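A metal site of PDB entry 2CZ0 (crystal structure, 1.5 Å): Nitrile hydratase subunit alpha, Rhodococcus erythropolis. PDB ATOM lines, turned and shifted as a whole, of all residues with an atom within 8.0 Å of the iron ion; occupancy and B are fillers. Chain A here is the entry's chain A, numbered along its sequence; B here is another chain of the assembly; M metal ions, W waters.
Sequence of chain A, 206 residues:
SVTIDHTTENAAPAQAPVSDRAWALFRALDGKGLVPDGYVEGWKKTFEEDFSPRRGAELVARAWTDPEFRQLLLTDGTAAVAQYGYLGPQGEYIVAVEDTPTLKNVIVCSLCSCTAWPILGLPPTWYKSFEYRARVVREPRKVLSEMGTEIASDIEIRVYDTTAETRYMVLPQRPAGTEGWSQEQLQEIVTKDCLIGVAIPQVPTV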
ATOM      1  N   GLN A  90     -18.342   0.889 -13.735  1.00  0.00           N
ATOM      2  CA  GLN A  90     -19.434   1.169 -14.659  1.00  0.00           C
ATOM      3  C   GLN A  90     -19.401   2.642 -15.022  1.00  0.00           C
ATOM      4  O   GLN A  90     -20.386   3.251 -15.425  1.00  0.00           O
ATOM      5  CB  GLN A  90     -20.810   0.744 -14.121  1.00  0.00           C
ATOM      6  CG  GLN A  90     -20.959  -0.799 -14.180  1.00  0.00           C
ATOM      7  CD  GLN A  90     -21.309  -1.265 -15.572  1.00  0.00           C
ATOM      8  OE1 GLN A  90     -20.471  -1.284 -16.469  1.00  0.00           O
ATOM      9  NE2 GLN A  90     -22.558  -1.661 -15.782  1.00  0.00           N
ATOM     10  N   VAL A 108     -30.009   3.411 -23.243  1.00  0.00           N
ATOM     11  CA  VAL A 108     -30.514   2.120 -22.782  1.00  0.00           C
ATOM     12  C   VAL A 108     -29.386   1.111 -22.759  1.00  0.00           C
ATOM     13  O   VAL A 108     -28.335   1.281 -23.404  1.00  0.00           O
ATOM     14  CB  VAL A 108     -31.617   1.641 -23.730  1.00  0.00           C
ATOM     15  CG1 VAL A 108     -31.057   1.409 -25.124  1.00  0.00           C
ATOM     16  CG2 VAL A 108     -32.293   0.357 -23.222  1.00  0.00           C
ATOM     17  N   CYS A 109     -29.554  -0.018 -22.087  1.00  0.00           N
ATOM     18  CA  CYS A 109     -28.736  -1.191 -22.286  1.00  0.00           C
ATOM     19  C   CYS A 109     -29.699  -2.337 -22.663  1.00  0.00           C
ATOM     20  O   CYS A 109     -30.279  -2.946 -21.748  1.00  0.00           O
ATOM     21  CB  CYS A 109     -27.996  -1.559 -21.004  1.00  0.00           C
ATOM     22  SG  CYS A 109     -26.953  -3.028 -21.211  1.00  0.00           S
ATOM     23  N   SER A 110     -29.830  -2.525 -23.968  1.00  0.00           N
ATOM     24  CA  SER A 110     -30.859  -3.504 -24.359  1.00  0.00           C
ATOM     25  C   SER A 110     -30.491  -4.910 -23.911  1.00  0.00           C
ATOM     26  O   SER A 110     -31.362  -5.764 -23.706  1.00  0.00           O
ATOM     27  CB  SER A 110     -31.066  -3.466 -25.871  1.00  0.00           C
ATOM     28  OG  SER A 110     -29.975  -3.992 -26.588  1.00  0.00           O
ATOM     29  N   LEU A 111     -29.196  -5.195 -23.744  1.00  0.00           N
ATOM     30  CA  LEU A 111     -28.713  -6.529 -23.426  1.00  0.00           C
ATOM     31  C   LEU A 111     -28.671  -6.827 -21.936  1.00  0.00           C
ATOM     32  O   LEU A 111     -28.509  -7.981 -21.553  1.00  0.00           O
ATOM     33  CB  LEU A 111     -27.319  -6.756 -24.067  1.00  0.00           C
ATOM     34  CG  LEU A 111     -27.251  -6.699 -25.592  1.00  0.00           C
ATOM     35  CD1 LEU A 111     -25.781  -6.731 -26.045  1.00  0.00           C
ATOM     36  CD2 LEU A 111     -28.052  -7.813 -26.251  1.00  0.00           C
ATOM     37  N   CSD A 112     -28.820  -5.811 -21.068  1.00  0.00           N
ATOM     38  CA  CSD A 112     -28.804  -6.024 -19.609  1.00  0.00           C
ATOM     39  CB  CSD A 112     -27.444  -6.579 -19.139  1.00  0.00           C
ATOM     40  SG  CSD A 112     -25.980  -5.733 -19.802  1.00  0.00           S
ATOM     41  C   CSD A 112     -29.161  -4.752 -18.829  1.00  0.00           C
ATOM     42  O   CSD A 112     -30.354  -4.615 -18.546  1.00  0.00           O
ATOM     43  OD1 CSD A 112     -25.801  -5.996 -21.282  1.00  0.00           O
ATOM     44  OD2 CSD A 112     -24.903  -6.367 -19.042  1.00  0.00           O
ATOM     45  N   SER A 113     -28.182  -3.877 -18.540  1.00  0.00           N
ATOM     46  CA  SER A 113     -28.604  -2.785 -17.662  1.00  0.00           C
ATOM     47  C   SER A 113     -27.535  -1.670 -17.577  1.00  0.00           C
ATOM     48  O   SER A 113     -27.738  -0.738 -16.808  1.00  0.00           O
ATOM     49  CB  SER A 113     -28.907  -3.263 -16.253  1.00  0.00           C
ATOM     50  OG  SER A 113     -27.620  -3.626 -15.631  1.00  0.00           O
ATOM     51  N   CSD A 114     -26.490  -1.874 -18.377  1.00  0.00           N
ATOM     52  CA  CSD A 114     -25.380  -0.911 -18.321  1.00  0.00           C
ATOM     53  CB  CSD A 114     -24.450  -1.222 -19.518  1.00  0.00           C
ATOM     54  SG  CSD A 114     -24.236  -3.065 -19.476  1.00  0.00           S
ATOM     55  C   CSD A 114     -25.797   0.569 -18.331  1.00  0.00           C
ATOM     56  O   CSD A 114     -26.596   1.077 -19.103  1.00  0.00           O
ATOM     57  OD1 CSD A 114     -23.304  -3.277 -18.296  1.00  0.00           O
ATOM     58  OD2 CSD A 114     -23.494  -3.373 -20.681  1.00  0.00           O
ATOM     59  N   THR A 115     -25.181   1.235 -17.371  1.00  0.00           N
ATOM     60  CA  THR A 115     -25.473   2.568 -16.909  1.00  0.00           C
ATOM     61  C   THR A 115     -24.199   3.215 -16.333  1.00  0.00           C
ATOM     62  O   THR A 115     -23.483   2.454 -15.726  1.00  0.00           O
ATOM     63  CB  THR A 115     -26.457   2.457 -15.742  1.00  0.00           C
ATOM     64  OG1 THR A 115     -27.716   2.024 -16.279  1.00  0.00           O
ATOM     65  CG2 THR A 115     -26.726   3.773 -15.033  1.00  0.00           C
ATOM     66  N   TRP A 117     -22.975   4.293 -13.565  1.00  0.00           N
ATOM     67  CA  TRP A 117     -23.309   4.204 -12.153  1.00  0.00           C
ATOM     68  C   TRP A 117     -22.843   5.424 -11.344  1.00  0.00           C
ATOM     69  O   TRP A 117     -23.644   5.959 -10.579  1.00  0.00           O
ATOM     70  CB  TRP A 117     -22.726   2.960 -11.473  1.00  0.00           C
ATOM     71  CG  TRP A 117     -23.351   1.659 -11.865  1.00  0.00           C
ATOM     72  CD1 TRP A 117     -24.398   1.457 -12.734  1.00  0.00           C
ATOM     73  CD2 TRP A 117     -22.976   0.352 -11.383  1.00  0.00           C
ATOM     74  NE1 TRP A 117     -24.679   0.110 -12.817  1.00  0.00           N
ATOM     75  CE2 TRP A 117     -23.828  -0.584 -11.999  1.00  0.00           C
ATOM     76  CE3 TRP A 117     -22.009  -0.094 -10.490  1.00  0.00           C
ATOM     77  CZ2 TRP A 117     -23.732  -1.963 -11.752  1.00  0.00           C
ATOM     78  CZ3 TRP A 117     -21.906  -1.462 -10.236  1.00  0.00           C
ATOM     79  CH2 TRP A 117     -22.774  -2.366 -10.873  1.00  0.00           C
ATOM     80  N   PRO A 123     -28.988   1.802 -11.983  1.00  0.00           N
ATOM     81  CA  PRO A 123     -30.202   1.959 -12.796  1.00  0.00           C
ATOM     82  C   PRO A 123     -31.443   1.570 -11.999  1.00  0.00           C
ATOM     83  O   PRO A 123     -31.419   0.696 -11.157  1.00  0.00           O
ATOM     84  CB  PRO A 123     -29.969   0.953 -13.920  1.00  0.00           C
ATOM     85  CG  PRO A 123     -29.100  -0.083 -13.292  1.00  0.00           C
ATOM     86  CD  PRO A 123     -28.080   0.761 -12.522  1.00  0.00           C
ATOM     87  N   TYR A 127     -35.656   0.860 -15.918  1.00  0.00           N
ATOM     88  CA  TYR A 127     -34.662   0.871 -16.996  1.00  0.00           C
ATOM     89  C   TYR A 127     -34.143  -0.529 -17.315  1.00  0.00           C
ATOM     90  O   TYR A 127     -33.756  -0.823 -18.442  1.00  0.00           O
ATOM     91  CB  TYR A 127     -33.522   1.754 -16.537  1.00  0.00           C
ATOM     92  CG  TYR A 127     -32.314   1.910 -17.399  1.00  0.00           C
ATOM     93  CD1 TYR A 127     -31.229   1.014 -17.315  1.00  0.00           C
ATOM     94  CD2 TYR A 127     -32.231   2.974 -18.292  1.00  0.00           C
ATOM     95  CE1 TYR A 127     -30.103   1.137 -18.100  1.00  0.00           C
ATOM     96  CE2 TYR A 127     -31.089   3.090 -19.083  1.00  0.00           C
ATOM     97  CZ  TYR A 127     -30.060   2.199 -18.978  1.00  0.00           C
ATOM     98  OH  TYR A 127     -28.944   2.418 -19.784  1.00  0.00           O
ATOM     99  N   LYS A 128     -34.142  -1.410 -16.314  1.00  0.00           N
ATOM    100  CA  LYS A 128     -33.767  -2.809 -16.481  1.00  0.00           C
ATOM    101  C   LYS A 128     -34.952  -3.670 -16.944  1.00  0.00           C
ATOM    102  O   LYS A 128     -34.751  -4.869 -17.143  1.00  0.00           O
ATOM    103  CB  LYS A 128     -33.281  -3.366 -15.149  1.00  0.00           C
ATOM    104  CG  LYS A 128     -32.056  -2.586 -14.659  1.00  0.00           C
ATOM    105  CD  LYS A 128     -31.625  -2.945 -13.279  1.00  0.00           C
ATOM    106  CE  LYS A 128     -32.523  -2.498 -12.150  1.00  0.00           C
ATOM    107  NZ  LYS A 128     -31.901  -2.657 -10.790  1.00  0.00           N
ATOM    108  N   ARG A 133     -36.061  -2.298 -22.375  1.00  0.00           N
ATOM    109  CA  ARG A 133     -34.990  -2.895 -23.170  1.00  0.00           C
ATOM    110  C   ARG A 133     -35.438  -3.331 -24.553  1.00  0.00           C
ATOM    111  O   ARG A 133     -34.708  -3.242 -25.525  1.00  0.00           O
ATOM    112  CB  ARG A 133     -34.455  -4.110 -22.377  1.00  0.00           C
ATOM    113  CG  ARG A 133     -33.656  -3.702 -21.147  1.00  0.00           C
ATOM    114  CD  ARG A 133     -33.196  -4.875 -20.283  1.00  0.00           C
ATOM    115  NE  ARG A 133     -32.605  -5.906 -21.131  1.00  0.00           N
ATOM    116  CZ  ARG A 133     -32.435  -7.182 -20.806  1.00  0.00           C
ATOM    117  NH1 ARG A 133     -32.773  -7.635 -19.601  1.00  0.00           N
ATOM    118  NH2 ARG A 133     -31.900  -8.007 -21.695  1.00  0.00           N
ATOM    119  N   ASP A 161     -27.449   2.595 -27.471  1.00  0.00           N
ATOM    120  CA  ASP A 161     -27.498   1.293 -26.798  1.00  0.00           C
ATOM    121  C   ASP A 161     -26.130   1.026 -26.199  1.00  0.00           C
ATOM    122  O   ASP A 161     -25.131   0.949 -26.957  1.00  0.00           O
ATOM    123  CB  ASP A 161     -27.938   0.246 -27.805  1.00  0.00           C
ATOM    124  CG  ASP A 161     -28.418  -1.027 -27.108  1.00  0.00           C
ATOM    125  OD1 ASP A 161     -28.303  -1.202 -25.878  1.00  0.00           O
ATOM    126  OD2 ASP A 161     -28.909  -1.869 -27.903  1.00  0.00           O
ATOM    127  N   THR A 162     -26.080   0.855 -24.906  1.00  0.00           N
ATOM    128  CA  THR A 162     -24.826   0.686 -24.147  1.00  0.00           C
ATOM    129  C   THR A 162     -24.381  -0.766 -24.241  1.00  0.00           C
ATOM    130  O   THR A 162     -24.661  -1.586 -23.365  1.00  0.00           O
ATOM    131  CB  THR A 162     -25.066   1.109 -22.691  1.00  0.00           C
ATOM    132  OG1 THR A 162     -25.620   2.455 -22.648  1.00  0.00           O
ATOM    133  CG2 THR A 162     -23.741   1.127 -21.909  1.00  0.00           C
ATOM    134  N   THR A 163     -23.694  -1.082 -25.314  1.00  0.00           N
ATOM    135  CA  THR A 163     -23.288  -2.445 -25.617  1.00  0.00           C
ATOM    136  C   THR A 163     -21.841  -2.785 -25.337  1.00  0.00           C
ATOM    137  O   THR A 163     -21.455  -3.955 -25.439  1.00  0.00           O
ATOM    138  CB  THR A 163     -23.539  -2.723 -27.110  1.00  0.00           C
ATOM    139  OG1 THR A 163     -23.008  -1.664 -27.930  1.00  0.00           O
ATOM    140  CG2 THR A 163     -25.043  -2.743 -27.426  1.00  0.00           C
ATOM    141  N   ALA A 164     -21.008  -1.781 -25.008  1.00  0.00           N
ATOM    142  CA  ALA A 164     -19.605  -2.113 -24.711  1.00  0.00           C
ATOM    143  C   ALA A 164     -19.185  -1.376 -23.443  1.00  0.00           C
ATOM    144  O   ALA A 164     -19.856  -1.444 -22.414  1.00  0.00           O
ATOM    145  CB  ALA A 164     -18.745  -1.821 -25.915  1.00  0.00           C
ATOM    146  N   ARG A 167     -19.842   4.575 -21.353  1.00  0.00           N
ATOM    147  CA  ARG A 167     -20.964   4.837 -20.457  1.00  0.00           C
ATOM    148  C   ARG A 167     -21.419   6.270 -20.673  1.00  0.00           C
ATOM    149  O   ARG A 167     -20.630   7.227 -20.713  1.00  0.00           O
ATOM    150  CB  ARG A 167     -20.625   4.607 -18.989  1.00  0.00           C
ATOM    151  CG  ARG A 167     -20.303   3.130 -18.746  1.00  0.00           C
ATOM    152  CD  ARG A 167     -21.602   2.299 -18.678  1.00  0.00           C
ATOM    153  NE  ARG A 167     -21.204   0.898 -18.468  1.00  0.00           N
ATOM    154  CZ  ARG A 167     -20.798   0.061 -19.434  1.00  0.00           C
ATOM    155  NH1 ARG A 167     -20.767   0.455 -20.711  1.00  0.00           N
ATOM    156  NH2 ARG A 167     -20.446  -1.190 -19.141  1.00  0.00           N
ATOM    157  N   TYR B  37     -24.179  -7.499  -6.738  1.00  0.00           N
ATOM    158  CA  TYR B  37     -23.116  -6.661  -7.319  1.00  0.00           C
ATOM    159  C   TYR B  37     -21.862  -6.728  -6.447  1.00  0.00           C
ATOM    160  O   TYR B  37     -20.752  -6.760  -6.966  1.00  0.00           O
ATOM    161  CB  TYR B  37     -23.618  -5.231  -7.419  1.00  0.00           C
ATOM    162  CG  TYR B  37     -24.541  -4.870  -8.560  1.00  0.00           C
ATOM    163  CD1 TYR B  37     -24.869  -5.733  -9.583  1.00  0.00           C
ATOM    164  CD2 TYR B  37     -25.053  -3.571  -8.546  1.00  0.00           C
ATOM    165  CE1 TYR B  37     -25.717  -5.282 -10.579  1.00  0.00           C
ATOM    166  CE2 TYR B  37     -25.915  -3.119  -9.560  1.00  0.00           C
ATOM    167  CZ  TYR B  37     -26.218  -4.014 -10.558  1.00  0.00           C
ATOM    168  OH  TYR B  37     -27.071  -3.561 -11.568  1.00  0.00           O
ATOM    169  N   ARG B  56     -21.875 -11.429 -17.524  1.00  0.00           N
ATOM    170  CA  ARG B  56     -22.946 -11.184 -18.506  1.00  0.00           C
ATOM    171  C   ARG B  56     -23.294 -12.521 -19.192  1.00  0.00           C
ATOM    172  O   ARG B  56     -24.497 -12.833 -19.308  1.00  0.00           O
ATOM    173  CB  ARG B  56     -22.523 -10.163 -19.550  1.00  0.00           C
ATOM    174  CG  ARG B  56     -22.238  -8.754 -19.021  1.00  0.00           C
ATOM    175  CD  ARG B  56     -22.203  -7.726 -20.189  1.00  0.00           C
ATOM    176  NE  ARG B  56     -22.057  -6.402 -19.545  1.00  0.00           N
ATOM    177  CZ  ARG B  56     -20.876  -5.817 -19.308  1.00  0.00           C
ATOM    178  NH1 ARG B  56     -19.756  -6.413 -19.666  1.00  0.00           N
ATOM    179  NH2 ARG B  56     -20.866  -4.629 -18.702  1.00  0.00           N
ATOM    180  N   TYR B  72     -34.434  -8.875 -12.037  1.00  0.00           N
ATOM    181  CA  TYR B  72     -33.073  -8.482 -12.339  1.00  0.00           C
ATOM    182  C   TYR B  72     -32.046  -8.916 -11.298  1.00  0.00           C
ATOM    183  O   TYR B  72     -31.086  -9.624 -11.628  1.00  0.00           O
ATOM    184  CB  TYR B  72     -33.034  -6.923 -12.465  1.00  0.00           C
ATOM    185  CG  TYR B  72     -31.624  -6.418 -12.709  1.00  0.00           C
ATOM    186  CD1 TYR B  72     -31.112  -6.402 -13.991  1.00  0.00           C
ATOM    187  CD2 TYR B  72     -30.809  -5.943 -11.680  1.00  0.00           C
ATOM    188  CE1 TYR B  72     -29.837  -5.949 -14.268  1.00  0.00           C
ATOM    189  CE2 TYR B  72     -29.527  -5.501 -11.900  1.00  0.00           C
ATOM    190  CZ  TYR B  72     -29.060  -5.512 -13.200  1.00  0.00           C
ATOM    191  OH  TYR B  72     -27.796  -5.072 -13.476  1.00  0.00           O
ATOM    192  N   TYR B  76     -28.634 -12.087 -11.168  1.00  0.00           N
ATOM    193  CA  TYR B  76     -27.194 -12.025 -10.869  1.00  0.00           C
ATOM    194  C   TYR B  76     -26.821 -12.823  -9.643  1.00  0.00           C
ATOM    195  O   TYR B  76     -25.679 -13.289  -9.558  1.00  0.00           O
ATOM    196  CB  TYR B  76     -26.794 -10.532 -10.719  1.00  0.00           C
ATOM    197  CG  TYR B  76     -26.881  -9.957 -12.133  1.00  0.00           C
ATOM    198  CD1 TYR B  76     -25.858  -9.961 -13.064  1.00  0.00           C
ATOM    199  CD2 TYR B  76     -28.118  -9.450 -12.503  1.00  0.00           C
ATOM    200  CE1 TYR B  76     -26.039  -9.427 -14.328  1.00  0.00           C
ATOM    201  CE2 TYR B  76     -28.317  -8.922 -13.754  1.00  0.00           C
ATOM    202  CZ  TYR B  76     -27.273  -8.917 -14.661  1.00  0.00           C
ATOM    203  OH  TYR B  76     -27.474  -8.397 -15.927  1.00  0.00           O
ATOM    204  N   ARG B 141     -21.233  -8.996 -27.968  1.00  0.00           N
ATOM    205  CA  ARG B 141     -21.862  -7.751 -27.578  1.00  0.00           C
ATOM    206  C   ARG B 141     -22.354  -7.020 -28.801  1.00  0.00           C
ATOM    207  O   ARG B 141     -22.200  -5.835 -29.013  1.00  0.00           O
ATOM    208  CB  ARG B 141     -20.818  -6.889 -26.814  1.00  0.00           C
ATOM    209  CG  ARG B 141     -20.508  -7.500 -25.455  1.00  0.00           C
ATOM    210  CD  ARG B 141     -21.792  -7.661 -24.642  1.00  0.00           C
ATOM    211  NE  ARG B 141     -22.346  -6.362 -24.234  1.00  0.00           N
ATOM    212  CZ  ARG B 141     -23.402  -6.232 -23.440  1.00  0.00           C
ATOM    213  NH1 ARG B 141     -24.012  -7.345 -23.031  1.00  0.00           N
ATOM    214  NH2 ARG B 141     -23.841  -5.043 -23.081  1.00  0.00           N
HETATM  215 FE    FE M   1     -26.273  -3.662 -19.132  1.00  0.00          FE
HETATM  216  O   HOH W   1     -25.796  -4.278 -17.236  1.00  0.00           O
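The nearest printed residue that does not touch the iron ion is Arg 141 of chain B (4.8 Å).
The iron ion is bound by N of CSD 114, 2.0 Å away.
The backbone nitrogen (N) of Ser 113 binds the iron ion (2.0 Å).
Water W1 is bound to the iron ion (2.0 Å).
SG of CSD 114 binds the iron ion, 2.2 Å away.
The iron ion is bound by SG of CSD 112, at 2.2 Å.
The iron ion is bound by SG of Cys 109, at 2.3 Å.
Water W1 lies within hydrogen-bond range of the side-chain hydroxyl of Ser 113, OD1 of CSD 114 and OD2 of CSD 112.
OD1 of CSD 114 sits at hydrogen-bond distance from the side-chain amide nitrogen (NE2) of Gln 90 (3.1 Å).
NH2 of Arg 167 lies within salt-bridge range of OD1 of CSD 114.
OD1 of CSD 112 is in salt-bridge range of the guanidinium group of Arg 141 of chain B (2.8 Å).
The side-chain hydroxyl (OH) of Tyr 72 of chain B sits at hydrogen-bond distance from the side-chain hydroxyl (OG) of Ser 113 (2.6 Å).
The guanidinium group of Arg 56 of chain B lies within salt-bridge range of OD1 of CSD 114 (2.8 Å).
O of CSD 114 is in hydrogen-bond range of the side-chain hydroxyl of Tyr 127, 2.8 Å away.
OH of Tyr 127 sits at hydrogen-bond distance from N of Cys 109 (3.4 Å).
OD2 of CSD 114 is in salt-bridge range of NH2 of Arg 141 of chain B (2.9 Å).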
